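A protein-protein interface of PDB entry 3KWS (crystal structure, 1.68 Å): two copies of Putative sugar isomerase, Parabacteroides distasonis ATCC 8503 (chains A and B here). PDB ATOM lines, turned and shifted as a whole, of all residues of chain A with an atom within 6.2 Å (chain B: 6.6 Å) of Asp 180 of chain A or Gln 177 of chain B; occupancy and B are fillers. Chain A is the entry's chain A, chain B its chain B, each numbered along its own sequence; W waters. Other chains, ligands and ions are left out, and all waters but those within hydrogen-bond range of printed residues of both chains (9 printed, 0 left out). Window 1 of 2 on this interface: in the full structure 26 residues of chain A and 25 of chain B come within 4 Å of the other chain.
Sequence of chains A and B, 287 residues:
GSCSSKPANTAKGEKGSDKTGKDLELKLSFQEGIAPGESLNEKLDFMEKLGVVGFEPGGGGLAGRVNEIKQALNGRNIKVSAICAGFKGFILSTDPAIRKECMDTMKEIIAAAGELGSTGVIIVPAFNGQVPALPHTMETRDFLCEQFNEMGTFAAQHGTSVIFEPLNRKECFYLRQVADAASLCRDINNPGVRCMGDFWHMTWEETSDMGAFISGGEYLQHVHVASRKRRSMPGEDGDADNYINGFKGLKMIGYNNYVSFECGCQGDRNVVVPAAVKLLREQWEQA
NE2 of Gln 177 of chain B is in hydrogen-bond range of O of Ala 179 of chain A. OE1 of Gln 177 of chain B lies close to N of Asp 180 of chain A (3.4 Å). The side-chain amide nitrogen (NE2) of Gln 177 of chain A lies within hydrogen-bond range of the backbone carbonyl oxygen (O) of Ala 179 of chain B (3.0 Å). OE1 of Gln 177 of chain A sits close to N of Asp 180 of chain B (3.4 Å).
The guanidinium group of Arg 141 of chain A sits at hydrogen-bond distance from the side-chain hydroxyl of Ser 183 of chain A (3.2 Å). NH1 of Arg 176 of chain B lies within salt-bridge range of OE1 of Glu 205 of chain B (3.4 Å). The side-chain amide nitrogen of Gln 177 of chain B lies within hydrogen-bond range of the backbone carbonyl oxygen of Glu 205 of chain B, at 2.9 Å.
NH1 of Arg 176 of chain B touches NE of Arg 141 of chain A, 3.6 Å away. Ala 182 of chain A touches Thr 207 of chain B. Ser 183 of chain A touches Gln 177 of chain B. O of Glu 205 of chain B touches OG of Ser 183 of chain A, 3.9 Å away. Ser 183 of chain A touches Thr 207 of chain B.
Asp 180 of chain A touches one residue of chain B. Gln 177 of chain B touches just these residues of chain A: Ala 179 (3.0 Å), Asp 180 (3.2 Å) and Ser 183 (3.8 Å). Of the printed residues of chain A, Glu 205 of chain B touches Ser 183. Printed residues of chain B within 4 Å of Ala 179 of chain A: Gln 177 (3.0 Å). Of the printed residues of chain A, Ala 179 of chain B touches Gln 177 (3.0 Å). Met 196 of chain B touches none of the printed residues of chain A. Leu 184 of chain A touches none of the printed residues of chain B. The nearest residue of chain A that does not touch Gln 177 of chain B is Ala 181 of chain A (5.6 Å). The nearest printed residue of chain A that does not touch Thr 207 of chain B is Ala 179 of chain A (4.9 Å).
Hydrophobic or aromatic side chains of chain A that line the printed part of chain B: Ala 179 and Ala 182. Of the 15 printed residues of chain B, 6 touch a printed residue of chain A. Among the printed residues, no Asp or Glu carboxylate lies within 4 Å of a Lys or Arg side-chain nitrogen of the other chain.
Gln 177 of chain A touches Ala 179 of chain B, and with the chains exchanged Ala 179 of chain A touches Gln 177 of chain B. Gln 177 of chain A touches Asp 180 of chain B, and with the chains exchanged Asp 180 of chain A touches Gln 177 of chain B.
Water W9 lies within hydrogen-bond range of the side-chain carboxylate of Glu 205 of chain B (2.6 Å), the side-chain hydroxyl of Ser 183 of chain A (2.8 Å) and the side-chain amide nitrogen of Gln 177 of chain B (3.4 Å). Water W7 lies within hydrogen-bond range of OD1 of Asp 180 of chain A, NH2 of Arg 141 of chain A, NH1 of Arg 176 of chain B and OG of Ser 183 of chain A. Water W4 bridges the side-chain carboxylate of Asp 180 of chain B (2.7 Å) and the guanidinium group of Arg 176 of chain A (3.0 Å). Water W8 lies within hydrogen-bond range of OD1 of Asp 180 of chain A (2.7 Å), NE of Arg 141 of chain A (2.9 Å) and NH2 of Arg 176 of chain B (3.0 Å). Water W5 lies within hydrogen-bond range of OG1 of Thr 207 of chain B, O of Ala 179 of chain A and NE2 of Gln 177 of chain B. Water W6 bridges the side-chain amide oxygen of Gln 177 of chain A (3.0 Å) and the side-chain amide oxygen of Gln 177 of chain B (3.1 Å).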
ATOM      1  N   HIS A 136      -5.387  -6.031  17.314  1.00  0.00           N
ATOM      2  CA  HIS A 136      -6.793  -5.683  17.411  1.00  0.00           C
ATOM      3  C   HIS A 136      -7.483  -6.830  18.184  1.00  0.00           C
ATOM      4  O   HIS A 136      -8.025  -7.784  17.613  1.00  0.00           O
ATOM      5  CB  HIS A 136      -7.420  -5.380  16.027  1.00  0.00           C
ATOM      6  CG  HIS A 136      -8.753  -4.706  16.088  1.00  0.00           C
ATOM      7  ND1 HIS A 136      -9.320  -4.265  17.258  1.00  0.00           N
ATOM      8  CD2 HIS A 136      -9.613  -4.338  15.101  1.00  0.00           C
ATOM      9  CE1 HIS A 136     -10.486  -3.694  17.008  1.00  0.00           C
ATOM     10  NE2 HIS A 136     -10.679  -3.711  15.702  1.00  0.00           N
ATOM     11  N   ARG A 141      -8.473  -3.150  23.123  1.00  0.00           N
ATOM     12  CA  ARG A 141      -9.647  -2.284  23.223  1.00  0.00           C
ATOM     13  C   ARG A 141      -9.793  -1.755  24.647  1.00  0.00           C
ATOM     14  O   ARG A 141     -10.038  -0.581  24.866  1.00  0.00           O
ATOM     15  CB  ARG A 141     -10.908  -3.005  22.784  1.00  0.00           C
ATOM     16  CG  ARG A 141     -12.102  -2.062  22.603  1.00  0.00           C
ATOM     17  CD  ARG A 141     -13.343  -2.839  22.289  1.00  0.00           C
ATOM     18  NE  ARG A 141     -14.518  -2.058  21.962  1.00  0.00           N
ATOM     19  CZ  ARG A 141     -15.371  -1.512  22.827  1.00  0.00           C
ATOM     20  NH1 ARG A 141     -15.186  -1.593  24.151  1.00  0.00           N
ATOM     21  NH2 ARG A 141     -16.429  -0.875  22.345  1.00  0.00           N
ATOM     22  N   TYR A 174      -7.976  -0.267  12.137  1.00  0.00           N
ATOM     23  CA  TYR A 174      -8.380  -0.388  13.532  1.00  0.00           C
ATOM     24  C   TYR A 174      -9.802   0.123  13.818  1.00  0.00           C
ATOM     25  O   TYR A 174     -10.602  -0.597  14.396  1.00  0.00           O
ATOM     26  CB  TYR A 174      -7.343   0.276  14.480  1.00  0.00           C
ATOM     27  CG  TYR A 174      -7.632  -0.036  15.914  1.00  0.00           C
ATOM     28  CD1 TYR A 174      -8.487   0.761  16.656  1.00  0.00           C
ATOM     29  CD2 TYR A 174      -7.156  -1.199  16.509  1.00  0.00           C
ATOM     30  CE1 TYR A 174      -8.837   0.416  17.946  1.00  0.00           C
ATOM     31  CE2 TYR A 174      -7.496  -1.546  17.824  1.00  0.00           C
ATOM     32  CZ  TYR A 174      -8.340  -0.711  18.545  1.00  0.00           C
ATOM     33  OH  TYR A 174      -8.738  -1.049  19.813  1.00  0.00           O
ATOM     34  N   LEU A 175     -10.100   1.358  13.404  1.00  0.00           N
ATOM     35  CA  LEU A 175     -11.390   1.978  13.670  1.00  0.00           C
ATOM     36  C   LEU A 175     -11.901   2.615  12.372  1.00  0.00           C
ATOM     37  O   LEU A 175     -11.357   3.598  11.870  1.00  0.00           O
ATOM     38  CB  LEU A 175     -11.275   3.001  14.811  1.00  0.00           C
ATOM     39  CG  LEU A 175     -12.539   3.811  15.091  1.00  0.00           C
ATOM     40  CD1 LEU A 175     -13.758   2.962  15.514  1.00  0.00           C
ATOM     41  CD2 LEU A 175     -12.194   4.848  16.204  1.00  0.00           C
ATOM     42  N   ARG A 176     -12.920   1.977  11.814  1.00  0.00           N
ATOM     43  CA  ARG A 176     -13.488   2.316  10.489  1.00  0.00           C
ATOM     44  C   ARG A 176     -14.942   2.786  10.460  1.00  0.00           C
ATOM     45  O   ARG A 176     -15.353   3.401   9.482  1.00  0.00           O
ATOM     46  CB  ARG A 176     -13.324   1.092   9.592  1.00  0.00           C
ATOM     47  CG  ARG A 176     -11.834   0.800   9.213  1.00  0.00           C
ATOM     48  CD  ARG A 176     -11.675  -0.447   8.402  1.00  0.00           C
ATOM     49  NE  ARG A 176     -11.950  -1.637   9.247  1.00  0.00           N
ATOM     50  CZ  ARG A 176     -12.926  -2.518   9.080  1.00  0.00           C
ATOM     51  NH1 ARG A 176     -13.743  -2.457   8.023  1.00  0.00           N
ATOM     52  NH2 ARG A 176     -13.039  -3.485   9.972  1.00  0.00           N
ATOM     53  N   GLN A 177     -15.750   2.448  11.477  1.00  0.00           N
ATOM     54  CA  GLN A 177     -17.154   2.781  11.508  1.00  0.00           C
ATOM     55  C   GLN A 177     -17.590   3.614  12.713  1.00  0.00           C
ATOM     56  O   GLN A 177     -17.108   3.421  13.852  1.00  0.00           O
ATOM     57  CB  GLN A 177     -17.980   1.515  11.482  1.00  0.00           C
ATOM     58  CG  GLN A 177     -17.790   0.779  10.159  1.00  0.00           C
ATOM     59  CD  GLN A 177     -18.590  -0.487  10.047  1.00  0.00           C
ATOM     60  OE1 GLN A 177     -18.319  -1.483  10.747  1.00  0.00           O
ATOM     61  NE2 GLN A 177     -19.590  -0.465   9.164  1.00  0.00           N
ATOM     62  N   VAL A 178     -18.599   4.437  12.472  1.00  0.00           N
ATOM     63  CA  VAL A 178     -19.160   5.320  13.491  1.00  0.00           C
ATOM     64  C   VAL A 178     -19.755   4.517  14.645  1.00  0.00           C
ATOM     65  O   VAL A 178     -19.536   4.865  15.811  1.00  0.00           O
ATOM     66  CB  VAL A 178     -20.192   6.350  12.923  1.00  0.00           C
ATOM     67  CG1 VAL A 178     -20.719   7.230  14.045  1.00  0.00           C
ATOM     68  CG2 VAL A 178     -19.539   7.242  11.806  1.00  0.00           C
ATOM     69  N   ALA A 179     -20.459   3.436  14.359  1.00  0.00           N
ATOM     70  CA  ALA A 179     -21.072   2.613  15.447  1.00  0.00           C
ATOM     71  C   ALA A 179     -20.005   2.054  16.381  1.00  0.00           C
ATOM     72  O   ALA A 179     -20.216   1.950  17.566  1.00  0.00           O
ATOM     73  CB  ALA A 179     -21.937   1.467  14.926  1.00  0.00           C
ATOM     74  N   ASP A 180     -18.865   1.687  15.834  1.00  0.00           N
ATOM     75  CA  ASP A 180     -17.731   1.175  16.637  1.00  0.00           C
ATOM     76  C   ASP A 180     -17.207   2.289  17.552  1.00  0.00           C
ATOM     77  O   ASP A 180     -17.049   2.099  18.764  1.00  0.00           O
ATOM     78  CB  ASP A 180     -16.671   0.637  15.699  1.00  0.00           C
ATOM     79  CG  ASP A 180     -15.591  -0.171  16.401  1.00  0.00           C
ATOM     80  OD1 ASP A 180     -15.735  -0.519  17.603  1.00  0.00           O
ATOM     81  OD2 ASP A 180     -14.588  -0.445  15.711  1.00  0.00           O
ATOM     82  N   ALA A 181     -16.962   3.454  16.972  1.00  0.00           N
ATOM     83  CA  ALA A 181     -16.500   4.619  17.765  1.00  0.00           C
ATOM     84  C   ALA A 181     -17.495   4.985  18.855  1.00  0.00           C
ATOM     85  O   ALA A 181     -17.098   5.294  19.998  1.00  0.00           O
ATOM     86  CB  ALA A 181     -16.230   5.838  16.833  1.00  0.00           C
ATOM     87  N   ALA A 182     -18.791   4.918  18.529  1.00  0.00           N
ATOM     88  CA  ALA A 182     -19.850   5.262  19.511  1.00  0.00           C
ATOM     89  C   ALA A 182     -19.905   4.270  20.659  1.00  0.00           C
ATOM     90  O   ALA A 182     -20.074   4.649  21.825  1.00  0.00           O
ATOM     91  CB  ALA A 182     -21.226   5.360  18.798  1.00  0.00           C
ATOM     92  N   SER A 183     -19.678   3.003  20.354  1.00  0.00           N
ATOM     93  CA  SER A 183     -19.675   1.978  21.402  1.00  0.00           C
ATOM     94  C   SER A 183     -18.453   2.188  22.324  1.00  0.00           C
ATOM     95  O   SER A 183     -18.521   2.010  23.540  1.00  0.00           O
ATOM     96  CB  SER A 183     -19.667   0.619  20.774  1.00  0.00           C
ATOM     97  OG  SER A 183     -19.545  -0.335  21.788  1.00  0.00           O
ATOM     98  N   LEU A 184     -17.325   2.580  21.742  1.00  0.00           N
ATOM     99  CA  LEU A 184     -16.144   2.905  22.552  1.00  0.00           C
ATOM    100  C   LEU A 184     -16.539   4.035  23.470  1.00  0.00           C
ATOM    101  O   LEU A 184     -16.261   3.976  24.653  1.00  0.00           O
ATOM    102  CB  LEU A 184     -14.931   3.311  21.700  1.00  0.00           C
ATOM    103  CG  LEU A 184     -14.241   2.207  20.896  1.00  0.00           C
ATOM    104  CD1 LEU A 184     -13.396   2.711  19.729  1.00  0.00           C
ATOM    105  CD2 LEU A 184     -13.376   1.386  21.889  1.00  0.00           C
ATOM    106  N   CYS A 185     -17.171   5.079  22.937  1.00  0.00           N
ATOM    107  CA  CYS A 185     -17.574   6.196  23.783  1.00  0.00           C
ATOM    108  C   CYS A 185     -18.527   5.777  24.899  1.00  0.00           C
ATOM    109  O   CYS A 185     -18.382   6.236  26.046  1.00  0.00           O
ATOM    110  CB  CYS A 185     -18.216   7.318  22.964  1.00  0.00           C
ATOM    111  SG  CYS A 185     -17.051   8.109  21.864  1.00  0.00           S
ATOM    112  N   PRO B 166     -23.354 -11.237  14.456  1.00  0.00           N
ATOM    113  CA  PRO B 166     -22.482 -10.597  15.440  1.00  0.00           C
ATOM    114  C   PRO B 166     -22.845 -10.984  16.866  1.00  0.00           C
ATOM    115  O   PRO B 166     -24.040 -11.074  17.223  1.00  0.00           O
ATOM    116  CB  PRO B 166     -22.747  -9.064  15.223  1.00  0.00           C
ATOM    117  CG  PRO B 166     -23.652  -8.997  14.061  1.00  0.00           C
ATOM    118  CD  PRO B 166     -24.368 -10.287  13.966  1.00  0.00           C
ATOM    119  N   LEU B 167     -21.821 -11.216  17.686  1.00  0.00           N
ATOM    120  CA  LEU B 167     -22.047 -11.569  19.069  1.00  0.00           C
ATOM    121  C   LEU B 167     -21.374 -10.563  19.978  1.00  0.00           C
ATOM    122  O   LEU B 167     -20.498  -9.796  19.540  1.00  0.00           O
ATOM    123  CB  LEU B 167     -21.421 -12.946  19.420  1.00  0.00           C
ATOM    124  CG  LEU B 167     -21.743 -14.149  18.514  1.00  0.00           C
ATOM    125  CD1 LEU B 167     -21.169 -15.435  19.128  1.00  0.00           C
ATOM    126  CD2 LEU B 167     -23.271 -14.231  18.280  1.00  0.00           C
ATOM    127  N   LEU B 175     -16.426 -10.196  15.329  1.00  0.00           N
ATOM    128  CA  LEU B 175     -17.590  -9.527  14.716  1.00  0.00           C
ATOM    129  C   LEU B 175     -18.662  -9.344  15.775  1.00  0.00           C
ATOM    130  O   LEU B 175     -19.282 -10.285  16.215  1.00  0.00           O
ATOM    131  CB  LEU B 175     -18.121 -10.333  13.508  1.00  0.00           C
ATOM    132  CG  LEU B 175     -19.412  -9.830  12.830  1.00  0.00           C
ATOM    133  CD1 LEU B 175     -19.205  -8.434  12.264  1.00  0.00           C
ATOM    134  CD2 LEU B 175     -19.871 -10.785  11.697  1.00  0.00           C
ATOM    135  N   ARG B 176     -18.839  -8.092  16.160  1.00  0.00           N
ATOM    136  CA  ARG B 176     -19.695  -7.700  17.253  1.00  0.00           C
ATOM    137  C   ARG B 176     -20.872  -6.783  16.909  1.00  0.00           C
ATOM    138  O   ARG B 176     -21.817  -6.722  17.724  1.00  0.00           O
ATOM    139  CB  ARG B 176     -18.832  -6.991  18.322  1.00  0.00           C
ATOM    140  CG  ARG B 176     -17.888  -7.970  19.082  1.00  0.00           C
ATOM    141  CD  ARG B 176     -16.901  -7.320  20.059  1.00  0.00           C
ATOM    142  NE  ARG B 176     -15.930  -6.569  19.286  1.00  0.00           N
ATOM    143  CZ  ARG B 176     -15.759  -5.256  19.273  1.00  0.00           C
ATOM    144  NH1 ARG B 176     -16.439  -4.439  20.074  1.00  0.00           N
ATOM    145  NH2 ARG B 176     -14.889  -4.769  18.438  1.00  0.00           N
ATOM    146  N   GLN B 177     -20.812  -6.083  15.775  1.00  0.00           N
ATOM    147  CA  GLN B 177     -21.836  -5.094  15.417  1.00  0.00           C
ATOM    148  C   GLN B 177     -22.455  -5.332  14.037  1.00  0.00           C
ATOM    149  O   GLN B 177     -21.818  -5.813  13.109  1.00  0.00           O
ATOM    150  CB  GLN B 177     -21.250  -3.706  15.466  1.00  0.00           C
ATOM    151  CG  GLN B 177     -20.860  -3.240  16.893  1.00  0.00           C
ATOM    152  CD  GLN B 177     -20.309  -1.861  16.923  1.00  0.00           C
ATOM    153  OE1 GLN B 177     -19.226  -1.607  16.379  1.00  0.00           O
ATOM    154  NE2 GLN B 177     -21.033  -0.944  17.563  1.00  0.00           N
ATOM    155  N   VAL B 178     -23.733  -5.006  13.964  1.00  0.00           N
ATOM    156  CA  VAL B 178     -24.518  -5.226  12.767  1.00  0.00           C
ATOM    157  C   VAL B 178     -23.947  -4.398  11.620  1.00  0.00           C
ATOM    158  O   VAL B 178     -23.862  -4.895  10.490  1.00  0.00           O
ATOM    159  CB  VAL B 178     -26.001  -4.872  12.998  1.00  0.00           C
ATOM    160  CG1 VAL B 178     -26.815  -5.023  11.686  1.00  0.00           C
ATOM    161  CG2 VAL B 178     -26.588  -5.715  14.136  1.00  0.00           C
ATOM    162  N   ALA B 179     -23.551  -3.141  11.887  1.00  0.00           N
ATOM    163  CA  ALA B 179     -22.983  -2.285  10.832  1.00  0.00           C
ATOM    164  C   ALA B 179     -21.740  -2.920  10.196  1.00  0.00           C
ATOM    165  O   ALA B 179     -21.518  -2.780   8.975  1.00  0.00           O
ATOM    166  CB  ALA B 179     -22.673  -0.867  11.317  1.00  0.00           C
ATOM    167  N   ASP B 180     -20.958  -3.627  11.025  1.00  0.00           N
ATOM    168  CA  ASP B 180     -19.748  -4.293  10.545  1.00  0.00           C
ATOM    169  C   ASP B 180     -20.194  -5.450   9.628  1.00  0.00           C
ATOM    170  O   ASP B 180     -19.693  -5.595   8.510  1.00  0.00           O
ATOM    171  CB  ASP B 180     -18.899  -4.737  11.751  1.00  0.00           C
ATOM    172  CG  ASP B 180     -17.514  -5.250  11.386  1.00  0.00           C
ATOM    173  OD1 ASP B 180     -17.019  -5.033  10.247  1.00  0.00           O
ATOM    174  OD2 ASP B 180     -16.890  -5.888  12.300  1.00  0.00           O
ATOM    175  N   ALA B 181     -21.137  -6.255  10.114  1.00  0.00           N
ATOM    176  CA  ALA B 181     -21.624  -7.389   9.296  1.00  0.00           C
ATOM    177  C   ALA B 181     -22.205  -6.888   7.970  1.00  0.00           C
ATOM    178  O   ALA B 181     -22.024  -7.510   6.933  1.00  0.00           O
ATOM    179  CB  ALA B 181     -22.641  -8.237  10.089  1.00  0.00           C
ATOM    180  N   ALA B 182     -22.936  -5.780   8.003  1.00  0.00           N
ATOM    181  CA  ALA B 182     -23.582  -5.226   6.817  1.00  0.00           C
ATOM    182  C   ALA B 182     -22.552  -4.750   5.797  1.00  0.00           C
ATOM    183  O   ALA B 182     -22.730  -4.941   4.602  1.00  0.00           O
ATOM    184  CB  ALA B 182     -24.508  -4.057   7.201  1.00  0.00           C
ATOM    185  N   MET B 196     -27.451 -10.462  10.238  1.00  0.00           N
ATOM    186  CA  MET B 196     -28.519 -10.383  11.199  1.00  0.00           C
ATOM    187  C   MET B 196     -28.090  -9.584  12.418  1.00  0.00           C
ATOM    188  O   MET B 196     -26.910  -9.242  12.567  1.00  0.00           O
ATOM    189  CB  MET B 196     -28.949 -11.807  11.629  1.00  0.00           C
ATOM    190  CG  MET B 196     -27.943 -12.590  12.433  1.00  0.00           C
ATOM    191  SD  MET B 196     -28.693 -14.254  13.135  1.00  0.00           S
ATOM    192  CE  MET B 196     -29.790 -13.509  14.541  1.00  0.00           C
ATOM    193  N   GLU B 205     -23.424  -4.379  22.522  1.00  0.00           N
ATOM    194  CA  GLU B 205     -22.573  -3.886  21.433  1.00  0.00           C
ATOM    195  C   GLU B 205     -23.134  -2.762  20.588  1.00  0.00           C
ATOM    196  O   GLU B 205     -22.369  -2.151  19.847  1.00  0.00           O
ATOM    197  CB  GLU B 205     -22.222  -5.043  20.499  1.00  0.00           C
ATOM    198  CG  GLU B 205     -21.483  -6.213  21.156  1.00  0.00           C
ATOM    199  CD  GLU B 205     -20.230  -5.876  21.893  1.00  0.00           C
ATOM    200  OE1 GLU B 205     -19.498  -4.907  21.495  1.00  0.00           O
ATOM    201  OE2 GLU B 205     -19.948  -6.592  22.905  1.00  0.00           O
ATOM    202  N   GLU B 206     -24.400  -2.456  20.696  1.00  0.00           N
ATOM    203  CA  GLU B 206     -24.980  -1.364  19.918  1.00  0.00           C
ATOM    204  C   GLU B 206     -25.449  -0.251  20.805  1.00  0.00           C
ATOM    205  O   GLU B 206     -26.230  -0.473  21.730  1.00  0.00           O
ATOM    206  CB  GLU B 206     -26.190  -1.823  19.089  1.00  0.00           C
ATOM    207  CG  GLU B 206     -25.973  -3.054  18.213  1.00  0.00           C
ATOM    208  CD  GLU B 206     -24.989  -2.875  17.084  1.00  0.00           C
ATOM    209  OE1 GLU B 206     -24.636  -1.732  16.743  1.00  0.00           O
ATOM    210  OE2 GLU B 206     -24.626  -3.917  16.502  1.00  0.00           O
ATOM    211  N   THR B 207     -24.997   0.968  20.485  1.00  0.00           N
ATOM    212  CA  THR B 207     -25.503   2.135  21.141  1.00  0.00           C
ATOM    213  C   THR B 207     -26.909   2.419  20.687  1.00  0.00           C
ATOM    214  O   THR B 207     -27.671   3.073  21.419  1.00  0.00           O
ATOM    215  CB  THR B 207     -24.657   3.394  20.843  1.00  0.00           C
ATOM    216  OG1 THR B 207     -24.505   3.538  19.440  1.00  0.00           O
ATOM    217  CG2 THR B 207     -23.255   3.286  21.533  1.00  0.00           C
ATOM    218  N   ALA B 212     -28.282   0.377  14.140  1.00  0.00           N
ATOM    219  CA  ALA B 212     -27.718  -0.914  13.744  1.00  0.00           C
ATOM    220  C   ALA B 212     -28.558  -1.581  12.670  1.00  0.00           C
ATOM    221  O   ALA B 212     -28.027  -2.021  11.631  1.00  0.00           O
ATOM    222  CB  ALA B 212     -27.605  -1.875  14.939  1.00  0.00           C
HETATM  223  O   HOH W   1     -17.173  -2.359  13.759  1.00  0.00           O
HETATM  224  O   HOH W   2     -14.636  -5.675   9.266  1.00  0.00           O
HETATM  225  O   HOH W   3     -22.583  -0.621   7.653  1.00  0.00           O
HETATM  226  O   HOH W   4     -16.531  -3.483   8.097  1.00  0.00           O
HETATM  227  O   HOH W   5     -22.842   1.691  18.388  1.00  0.00           O
HETATM  228  O   HOH W   6     -19.657  -1.139  13.395  1.00  0.00           O
HETATM  229  O   HOH W   7     -17.155  -1.575  19.619  1.00  0.00           O
HETATM  230  O   HOH W   8     -14.028  -1.962  19.116  1.00  0.00           O
HETATM  231  O   HOH W   9     -19.639  -2.644  20.207  1.00  0.00           O
